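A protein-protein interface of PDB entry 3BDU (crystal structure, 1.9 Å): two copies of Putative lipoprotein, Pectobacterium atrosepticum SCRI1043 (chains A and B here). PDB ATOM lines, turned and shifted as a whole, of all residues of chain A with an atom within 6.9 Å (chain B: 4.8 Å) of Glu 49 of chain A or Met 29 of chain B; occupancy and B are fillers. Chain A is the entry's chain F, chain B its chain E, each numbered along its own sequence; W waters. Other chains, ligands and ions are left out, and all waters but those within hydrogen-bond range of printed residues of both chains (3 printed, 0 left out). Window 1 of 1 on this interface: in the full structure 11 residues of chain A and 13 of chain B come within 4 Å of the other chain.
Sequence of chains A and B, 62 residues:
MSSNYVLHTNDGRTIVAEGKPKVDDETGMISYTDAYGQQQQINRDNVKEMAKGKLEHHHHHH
Of chain B, only Arg 13 (2.6 Å), Met 29 (3.9 Å), Gln 41 (3.2 Å) and Ile 42 (3.97 Å) come within 4 Å of Glu 49 of chain A.
Of chain A, only Val 47 (3.9 Å), Lys 48 (3.8 Å) and Glu 49 (3.9 Å) come within 4 Å of Met 29 of chain B.
Of chain A, only Arg 44 comes within 4 Å of Gly 28 of chain B.
Of the printed residues of chain A, Arg 13 of chain B touches Glu 49.
Printed residues of chain A within 4 Å of Ile 42 of chain B: Lys 48 (3.5 Å) and Glu 49 (3.97 Å).
The nearest printed residue of chain A that does not touch Met 29 of chain B is Met 50 of chain A (4.2 Å).
OG1 of Thr 27 of chain B lies close to O of Asp 24 of chain B, 3.3 Å away.
The backbone NH of Asp 24 of chain B sits at hydrogen-bond distance from the backbone carbonyl oxygen of Met 29 of chain B.
OD2 of Asp 24 of chain B is in hydrogen-bond range of NE2 of Gln 41 of chain B (2.9 Å).
The backbone NH (N) of Met 29 of chain B lies within hydrogen-bond range of the side-chain hydroxyl (OG1) of Thr 27 of chain B (3.0 Å).
The backbone carbonyl oxygen (O) of His 8 of chain A is in hydrogen-bond range of the backbone NH (N) of Lys 48 of chain A.
The backbone carbonyl oxygen (O) of Glu 49 of chain A sits at hydrogen-bond distance from the backbone NH (N) of His 8 of chain A, 2.9 Å away.
Positions printed for both chains: 23, 30 and 46.
Water W2 bridges O of Gly 28 of chain B (2.8 Å) and NH2 of Arg 44 of chain A (3.1 Å).
Water W1 lies within hydrogen-bond range of the backbone carbonyl oxygen of Arg 44 of chain A (2.8 Å), the side-chain amide nitrogen of Asn 43 of chain B (3.2 Å) and the side-chain sulfur of Met 29 of chain B (3.6 Å).
Water W3 bridges the side-chain amide nitrogen (ND2) of Asn 43 of chain B (2.8 Å) and the backbone carbonyl oxygen (O) of Arg 44 of chain A (3.5 Å).
Of the 14 printed residues of chain A, 6 touch a printed residue of chain B.
Printed residues of chain A that touch a printed residue of chain B: Val 23, Arg 44, Val 47, Lys 48, Glu 49 and Met 50.
Among the printed residues, 15 pairs touch across the chains.
NH1 of Arg 13 of chain B is in salt-bridge range of OE2 of Glu 49 of chain A, 2.6 Å away.
NH2 of Arg 44 of chain A sits close to O of Gly 28 of chain B, at 3.4 Å.
N of Gln 41 of chain B lies within hydrogen-bond range of O of Met 50 of chain A, at 2.8 Å.
ND2 of Asn 43 of chain B sits at hydrogen-bond distance from O of Arg 44 of chain A, 3.1 Å away.
O of Val 47 of chain A lies within hydrogen-bond range of ND2 of Asn 43 of chain B, at 3.0 Å.
N of Asn 43 of chain B sits at hydrogen-bond distance from O of Lys 48 of chain A (3.0 Å).
Among the printed residues, pairs that only touch across the chains: Val 23 of chain A with Thr 27 of chain B, Arg 44 of chain A with Thr 27 of chain B, Val 47 of chain A with Met 29 of chain B, Lys 48 of chain A with Met 29 of chain B, Lys 48 of chain A with Ile 42 of chain B, Lys 48 of chain A with Asn 46 of chain B, Glu 49 of chain A with Met 29 of chain B, Glu 49 of chain A with Gln 41 of chain B and Glu 49 of chain A with Ile 42 of chain B.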
ATOM      1  N   VAL A   6       7.886  16.023  -0.602  1.00  0.00           N
ATOM      2  CA  VAL A   6       6.816  15.382   0.133  1.00  0.00           C
ATOM      3  C   VAL A   6       5.610  16.299   0.131  1.00  0.00           C
ATOM      4  O   VAL A   6       5.704  17.451   0.545  1.00  0.00           O
ATOM      5  CB  VAL A   6       7.227  15.109   1.590  1.00  0.00           C
ATOM      6  CG1 VAL A   6       6.058  14.508   2.352  1.00  0.00           C
ATOM      7  CG2 VAL A   6       8.425  14.163   1.624  1.00  0.00           C
ATOM      8  N   LEU A   7       4.484  15.785  -0.350  1.00  0.00           N
ATOM      9  CA  LEU A   7       3.246  16.553  -0.388  1.00  0.00           C
ATOM     10  C   LEU A   7       2.334  16.063   0.727  1.00  0.00           C
ATOM     11  O   LEU A   7       2.272  14.864   1.005  1.00  0.00           O
ATOM     12  CB  LEU A   7       2.512  16.369  -1.722  1.00  0.00           C
ATOM     13  CG  LEU A   7       3.201  16.722  -3.038  1.00  0.00           C
ATOM     14  CD1 LEU A   7       4.199  15.633  -3.398  1.00  0.00           C
ATOM     15  CD2 LEU A   7       2.163  16.848  -4.131  1.00  0.00           C
ATOM     16  N   HIS A   8       1.645  16.997   1.373  1.00  0.00           N
ATOM     17  CA  HIS A   8       0.700  16.661   2.429  1.00  0.00           C
ATOM     18  C   HIS A   8      -0.650  17.077   1.855  1.00  0.00           C
ATOM     19  O   HIS A   8      -0.843  18.241   1.510  1.00  0.00           O
ATOM     20  CB  HIS A   8       1.005  17.452   3.709  1.00  0.00           C
ATOM     21  CG  HIS A   8       2.278  17.045   4.388  1.00  0.00           C
ATOM     22  ND1 HIS A   8       2.820  17.751   5.441  1.00  0.00           N
ATOM     23  CD2 HIS A   8       3.121  16.009   4.159  1.00  0.00           C
ATOM     24  CE1 HIS A   8       3.943  17.171   5.828  1.00  0.00           C
ATOM     25  NE2 HIS A   8       4.148  16.112   5.067  1.00  0.00           N
ATOM     26  N   THR A   9      -1.569  16.126   1.719  1.00  0.00           N
ATOM     27  CA  THR A   9      -2.882  16.435   1.161  1.00  0.00           C
ATOM     28  C   THR A   9      -3.831  16.985   2.219  1.00  0.00           C
ATOM     29  O   THR A   9      -3.530  16.950   3.411  1.00  0.00           O
ATOM     30  CB  THR A   9      -3.533  15.190   0.528  1.00  0.00           C
ATOM     31  OG1 THR A   9      -3.800  14.215   1.545  1.00  0.00           O
ATOM     32  CG2 THR A   9      -2.613  14.586  -0.528  1.00  0.00           C
ATOM     33  N   ASN A  10      -4.969  17.517   1.784  1.00  0.00           N
ATOM     34  CA  ASN A  10      -5.940  18.036   2.735  1.00  0.00           C
ATOM     35  C   ASN A  10      -6.856  16.907   3.200  1.00  0.00           C
ATOM     36  O   ASN A  10      -7.821  17.145   3.923  1.00  0.00           O
ATOM     37  CB  ASN A  10      -6.774  19.174   2.129  1.00  0.00           C
ATOM     38  CG  ASN A  10      -6.083  20.530   2.225  1.00  0.00           C
ATOM     39  OD1 ASN A  10      -5.620  20.936   3.298  1.00  0.00           O
ATOM     40  ND2 ASN A  10      -6.025  21.244   1.105  1.00  0.00           N
ATOM     41  N   VAL A  23       2.516  23.101 -11.198  1.00  0.00           N
ATOM     42  CA  VAL A  23       1.221  23.156 -11.864  1.00  0.00           C
ATOM     43  C   VAL A  23       1.393  22.902 -13.356  1.00  0.00           C
ATOM     44  O   VAL A  23       2.302  23.439 -13.992  1.00  0.00           O
ATOM     45  CB  VAL A  23       0.540  24.533 -11.670  1.00  0.00           C
ATOM     46  CG1 VAL A  23      -0.849  24.534 -12.315  1.00  0.00           C
ATOM     47  CG2 VAL A  23       0.426  24.841 -10.196  1.00  0.00           C
ATOM     48  N   ILE A  30      -1.652  20.075  -9.982  1.00  0.00           N
ATOM     49  CA  ILE A  30      -0.254  19.900  -9.604  1.00  0.00           C
ATOM     50  C   ILE A  30       0.261  18.564 -10.130  1.00  0.00           C
ATOM     51  O   ILE A  30      -0.252  17.505  -9.773  1.00  0.00           O
ATOM     52  CB  ILE A  30      -0.093  19.962  -8.076  1.00  0.00           C
ATOM     53  CG1 ILE A  30      -0.377  21.388  -7.601  1.00  0.00           C
ATOM     54  CG2 ILE A  30       1.316  19.532  -7.675  1.00  0.00           C
ATOM     55  CD1 ILE A  30      -0.463  21.526  -6.105  1.00  0.00           C
ATOM     56  N   ARG A  44      -5.033  21.032  -6.920  1.00  0.00           N
ATOM     57  CA  ARG A  44      -4.308  21.898  -5.998  1.00  0.00           C
ATOM     58  C   ARG A  44      -5.075  22.185  -4.708  1.00  0.00           C
ATOM     59  O   ARG A  44      -4.472  22.440  -3.666  1.00  0.00           O
ATOM     60  CB  ARG A  44      -3.909  23.210  -6.684  1.00  0.00           C
ATOM     61  CG  ARG A  44      -5.047  23.966  -7.351  1.00  0.00           C
ATOM     62  CD  ARG A  44      -4.491  25.028  -8.294  1.00  0.00           C
ATOM     63  NE  ARG A  44      -3.802  26.099  -7.576  1.00  0.00           N
ATOM     64  CZ  ARG A  44      -2.907  26.913  -8.127  1.00  0.00           C
ATOM     65  NH1 ARG A  44      -2.581  26.780  -9.405  1.00  0.00           N
ATOM     66  NH2 ARG A  44      -2.346  27.872  -7.403  1.00  0.00           N
ATOM     67  N   ASN A  46      -6.453  20.113  -2.935  1.00  0.00           N
ATOM     68  CA  ASN A  46      -6.227  19.023  -1.993  1.00  0.00           C
ATOM     69  C   ASN A  46      -4.762  18.965  -1.564  1.00  0.00           C
ATOM     70  O   ASN A  46      -4.342  18.020  -0.897  1.00  0.00           O
ATOM     71  CB  ASN A  46      -6.626  17.661  -2.570  1.00  0.00           C
ATOM     72  CG  ASN A  46      -6.690  16.570  -1.493  1.00  0.00           C
ATOM     73  OD1 ASN A  46      -6.602  15.373  -1.787  1.00  0.00           O
ATOM     74  ND2 ASN A  46      -6.855  16.988  -0.238  1.00  0.00           N
ATOM     75  N   VAL A  47      -3.979  19.962  -1.965  1.00  0.00           N
ATOM     76  CA  VAL A  47      -2.574  20.008  -1.568  1.00  0.00           C
ATOM     77  C   VAL A  47      -2.426  21.112  -0.539  1.00  0.00           C
ATOM     78  O   VAL A  47      -2.597  22.293  -0.842  1.00  0.00           O
ATOM     79  CB  VAL A  47      -1.632  20.293  -2.750  1.00  0.00           C
ATOM     80  CG1 VAL A  47      -0.187  20.353  -2.243  1.00  0.00           C
ATOM     81  CG2 VAL A  47      -1.769  19.183  -3.806  1.00  0.00           C
ATOM     82  N   LYS A  48      -2.108  20.703   0.681  1.00  0.00           N
ATOM     83  CA  LYS A  48      -1.959  21.604   1.808  1.00  0.00           C
ATOM     84  C   LYS A  48      -0.560  22.170   1.941  1.00  0.00           C
ATOM     85  O   LYS A  48      -0.386  23.372   2.125  1.00  0.00           O
ATOM     86  CB  LYS A  48      -2.326  20.863   3.098  1.00  0.00           C
ATOM     87  CG  LYS A  48      -2.259  21.719   4.354  1.00  0.00           C
ATOM     88  CD  LYS A  48      -2.724  20.944   5.580  1.00  0.00           C
ATOM     89  CE  LYS A  48      -1.792  19.793   5.911  1.00  0.00           C
ATOM     90  NZ  LYS A  48      -2.280  19.037   7.098  1.00  0.00           N
ATOM     91  N   GLU A  49       0.432  21.291   1.859  1.00  0.00           N
ATOM     92  CA  GLU A  49       1.821  21.696   1.997  1.00  0.00           C
ATOM     93  C   GLU A  49       2.732  20.829   1.165  1.00  0.00           C
ATOM     94  O   GLU A  49       2.352  19.744   0.714  1.00  0.00           O
ATOM     95  CB  GLU A  49       2.283  21.579   3.447  1.00  0.00           C
ATOM     96  CG  GLU A  49       1.527  22.408   4.443  1.00  0.00           C
ATOM     97  CD  GLU A  49       2.023  22.154   5.850  1.00  0.00           C
ATOM     98  OE1 GLU A  49       2.011  20.979   6.281  1.00  0.00           O
ATOM     99  OE2 GLU A  49       2.430  23.122   6.523  1.00  0.00           O
ATOM    100  N   MET A  50       3.960  21.305   1.021  1.00  0.00           N
ATOM    101  CA  MET A  50       4.970  20.618   0.247  1.00  0.00           C
ATOM    102  C   MET A  50       6.336  20.918   0.862  1.00  0.00           C
ATOM    103  O   MET A  50       6.612  22.054   1.247  1.00  0.00           O
ATOM    104  CB  MET A  50       4.918  21.151  -1.173  1.00  0.00           C
ATOM    105  CG  MET A  50       5.467  20.242  -2.220  1.00  0.00           C
ATOM    106  SD  MET A  50       4.877  20.973  -3.886  1.00  0.00           S
ATOM    107  CE  MET A  50       3.143  20.153  -3.992  1.00  0.00           C
ATOM    108  N   ALA A  51       7.185  19.902   0.951  1.00  0.00           N
ATOM    109  CA  ALA A  51       8.516  20.092   1.516  1.00  0.00           C
ATOM    110  C   ALA A  51       9.573  19.382   0.669  1.00  0.00           C
ATOM    111  O   ALA A  51       9.363  18.263   0.194  1.00  0.00           O
ATOM    112  CB  ALA A  51       8.550  19.574   2.954  1.00  0.00           C
ATOM    113  N   ARG B  13      -1.033  26.059  13.332  1.00  0.00           N
ATOM    114  CA  ARG B  13       0.410  26.067  13.450  1.00  0.00           C
ATOM    115  C   ARG B  13       1.021  27.447  13.286  1.00  0.00           C
ATOM    116  O   ARG B  13       0.462  28.325  12.623  1.00  0.00           O
ATOM    117  CB  ARG B  13       1.033  25.129  12.413  1.00  0.00           C
ATOM    118  CG  ARG B  13       0.873  23.653  12.721  1.00  0.00           C
ATOM    119  CD  ARG B  13       1.413  22.830  11.572  1.00  0.00           C
ATOM    120  NE  ARG B  13       0.653  23.100  10.357  1.00  0.00           N
ATOM    121  CZ  ARG B  13       1.064  22.801   9.131  1.00  0.00           C
ATOM    122  NH1 ARG B  13       2.244  22.216   8.950  1.00  0.00           N
ATOM    123  NH2 ARG B  13       0.297  23.090   8.086  1.00  0.00           N
ATOM    124  N   ILE B  15       4.536  28.971  12.025  1.00  0.00           N
ATOM    125  CA  ILE B  15       5.723  28.560  11.291  1.00  0.00           C
ATOM    126  C   ILE B  15       6.670  29.732  11.069  1.00  0.00           C
ATOM    127  O   ILE B  15       6.243  30.821  10.696  1.00  0.00           O
ATOM    128  CB  ILE B  15       5.330  27.986   9.919  1.00  0.00           C
ATOM    129  CG1 ILE B  15       4.313  26.858  10.095  1.00  0.00           C
ATOM    130  CG2 ILE B  15       6.569  27.484   9.187  1.00  0.00           C
ATOM    131  CD1 ILE B  15       3.741  26.345   8.786  1.00  0.00           C
ATOM    132  N   LYS B  22       6.685  34.100  -0.396  1.00  0.00           N
ATOM    133  CA  LYS B  22       6.113  34.641  -1.635  1.00  0.00           C
ATOM    134  C   LYS B  22       5.536  33.537  -2.513  1.00  0.00           C
ATOM    135  O   LYS B  22       6.036  32.415  -2.512  1.00  0.00           O
ATOM    136  CB  LYS B  22       7.190  35.369  -2.441  1.00  0.00           C
ATOM    137  CG  LYS B  22       7.750  36.606  -1.754  1.00  0.00           C
ATOM    138  CD  LYS B  22       8.768  37.310  -2.635  1.00  0.00           C
ATOM    139  CE  LYS B  22       9.215  38.626  -2.007  1.00  0.00           C
ATOM    140  NZ  LYS B  22      10.010  39.467  -2.952  1.00  0.00           N
ATOM    141  N   VAL B  23       4.498  33.857  -3.279  1.00  0.00           N
ATOM    142  CA  VAL B  23       3.913  32.861  -4.155  1.00  0.00           C
ATOM    143  C   VAL B  23       4.928  32.436  -5.210  1.00  0.00           C
ATOM    144  O   VAL B  23       5.626  33.264  -5.798  1.00  0.00           O
ATOM    145  CB  VAL B  23       2.634  33.387  -4.850  1.00  0.00           C
ATOM    146  CG1 VAL B  23       2.132  32.364  -5.868  1.00  0.00           C
ATOM    147  CG2 VAL B  23       1.553  33.651  -3.803  1.00  0.00           C
ATOM    148  N   ASP B  24       5.019  31.128  -5.419  1.00  0.00           N
ATOM    149  CA  ASP B  24       5.913  30.549  -6.412  1.00  0.00           C
ATOM    150  C   ASP B  24       5.051  30.424  -7.667  1.00  0.00           C
ATOM    151  O   ASP B  24       4.065  29.699  -7.668  1.00  0.00           O
ATOM    152  CB  ASP B  24       6.373  29.163  -5.949  1.00  0.00           C
ATOM    153  CG  ASP B  24       7.249  28.452  -6.974  1.00  0.00           C
ATOM    154  OD1 ASP B  24       7.224  28.820  -8.172  1.00  0.00           O
ATOM    155  OD2 ASP B  24       7.961  27.506  -6.575  1.00  0.00           O
ATOM    156  N   THR B  27       3.912  26.902  -8.872  1.00  0.00           N
ATOM    157  CA  THR B  27       3.099  26.037  -8.008  1.00  0.00           C
ATOM    158  C   THR B  27       1.794  26.698  -7.582  1.00  0.00           C
ATOM    159  O   THR B  27       0.816  26.017  -7.273  1.00  0.00           O
ATOM    160  CB  THR B  27       3.810  25.666  -6.700  1.00  0.00           C
ATOM    161  OG1 THR B  27       4.008  26.853  -5.927  1.00  0.00           O
ATOM    162  CG2 THR B  27       5.141  24.983  -6.969  1.00  0.00           C
ATOM    163  N   GLY B  28       1.791  28.025  -7.545  1.00  0.00           N
ATOM    164  CA  GLY B  28       0.608  28.742  -7.120  1.00  0.00           C
ATOM    165  C   GLY B  28       0.526  28.768  -5.606  1.00  0.00           C
ATOM    166  O   GLY B  28      -0.405  29.331  -5.041  1.00  0.00           O
ATOM    167  N   MET B  29       1.511  28.170  -4.942  1.00  0.00           N
ATOM    168  CA  MET B  29       1.512  28.126  -3.479  1.00  0.00           C
ATOM    169  C   MET B  29       2.513  29.111  -2.886  1.00  0.00           C
ATOM    170  O   MET B  29       3.353  29.657  -3.604  1.00  0.00           O
ATOM    171  CB  MET B  29       1.832  26.701  -3.017  1.00  0.00           C
ATOM    172  CG  MET B  29       0.792  25.668  -3.460  1.00  0.00           C
ATOM    173  SD  MET B  29       1.403  23.852  -3.147  1.00  0.00           S
ATOM    174  CE  MET B  29       1.289  23.843  -1.227  1.00  0.00           C
ATOM    175  N   ILE B  30       2.410  29.355  -1.581  1.00  0.00           N
ATOM    176  CA  ILE B  30       3.327  30.272  -0.914  1.00  0.00           C
ATOM    177  C   ILE B  30       4.599  29.507  -0.575  1.00  0.00           C
ATOM    178  O   ILE B  30       4.565  28.513   0.149  1.00  0.00           O
ATOM    179  CB  ILE B  30       2.692  30.856   0.354  1.00  0.00           C
ATOM    180  CG1 ILE B  30       1.544  31.792  -0.047  1.00  0.00           C
ATOM    181  CG2 ILE B  30       3.738  31.619   1.157  1.00  0.00           C
ATOM    182  CD1 ILE B  30       0.710  32.276   1.109  1.00  0.00           C
ATOM    183  N   SER B  31       5.715  29.970  -1.129  1.00  0.00           N
ATOM    184  CA  SER B  31       7.016  29.337  -0.946  1.00  0.00           C
ATOM    185  C   SER B  31       7.889  30.083   0.056  1.00  0.00           C
ATOM    186  O   SER B  31       7.919  31.312   0.069  1.00  0.00           O
ATOM    187  CB  SER B  31       7.752  29.267  -2.290  1.00  0.00           C
ATOM    188  OG  SER B  31       9.110  28.889  -2.131  1.00  0.00           O
ATOM    189  N   GLN B  41       6.450  24.796   0.931  1.00  0.00           N
ATOM    190  CA  GLN B  41       5.417  25.533   0.224  1.00  0.00           C
ATOM    191  C   GLN B  41       4.111  25.238   0.931  1.00  0.00           C
ATOM    192  O   GLN B  41       3.895  24.127   1.416  1.00  0.00           O
ATOM    193  CB  GLN B  41       5.324  25.095  -1.244  1.00  0.00           C
ATOM    194  CG  GLN B  41       6.629  25.219  -2.012  1.00  0.00           C
ATOM    195  CD  GLN B  41       6.457  25.955  -3.333  1.00  0.00           C
ATOM    196  OE1 GLN B  41       5.341  26.326  -3.711  1.00  0.00           O
ATOM    197  NE2 GLN B  41       7.565  26.180  -4.036  1.00  0.00           N
ATOM    198  N   ILE B  42       3.243  26.236   1.012  1.00  0.00           N
ATOM    199  CA  ILE B  42       1.963  26.034   1.662  1.00  0.00           C
ATOM    200  C   ILE B  42       0.860  26.694   0.844  1.00  0.00           C
ATOM    201  O   ILE B  42       1.062  27.758   0.261  1.00  0.00           O
ATOM    202  CB  ILE B  42       1.981  26.594   3.106  1.00  0.00           C
ATOM    203  CG1 ILE B  42       0.671  26.247   3.820  1.00  0.00           C
ATOM    204  CG2 ILE B  42       2.216  28.100   3.081  1.00  0.00           C
ATOM    205  CD1 ILE B  42       0.715  26.498   5.320  1.00  0.00           C
ATOM    206  N   ASN B  43      -0.291  26.034   0.783  1.00  0.00           N
ATOM    207  CA  ASN B  43      -1.438  26.539   0.037  1.00  0.00           C
ATOM    208  C   ASN B  43      -1.890  27.841   0.686  1.00  0.00           C
ATOM    209  O   ASN B  43      -2.068  27.900   1.905  1.00  0.00           O
ATOM    210  CB  ASN B  43      -2.573  25.506   0.091  1.00  0.00           C
ATOM    211  CG  ASN B  43      -3.675  25.785  -0.919  1.00  0.00           C
ATOM    212  OD1 ASN B  43      -4.230  26.873  -0.957  1.00  0.00           O
ATOM    213  ND2 ASN B  43      -3.996  24.789  -1.738  1.00  0.00           N
ATOM    214  N   ASN B  46      -4.436  27.837   3.250  1.00  0.00           N
ATOM    215  CA  ASN B  46      -4.122  27.315   4.579  1.00  0.00           C
ATOM    216  C   ASN B  46      -3.393  28.356   5.425  1.00  0.00           C
ATOM    217  O   ASN B  46      -3.031  28.086   6.569  1.00  0.00           O
ATOM    218  CB  ASN B  46      -3.254  26.058   4.476  1.00  0.00           C
ATOM    219  CG  ASN B  46      -3.010  25.399   5.830  1.00  0.00           C
ATOM    220  OD1 ASN B  46      -2.049  24.640   6.001  1.00  0.00           O
ATOM    221  ND2 ASN B  46      -3.882  25.675   6.793  1.00  0.00           N
HETATM  222  O   HOH W   1      -2.038  23.829  -4.147  1.00  0.00           O
HETATM  223  O   HOH W   2      -2.265  30.818  -6.483  1.00  0.00           O
HETATM  224  O   HOH W   3      -6.017  25.551  -3.596  1.00  0.00           O
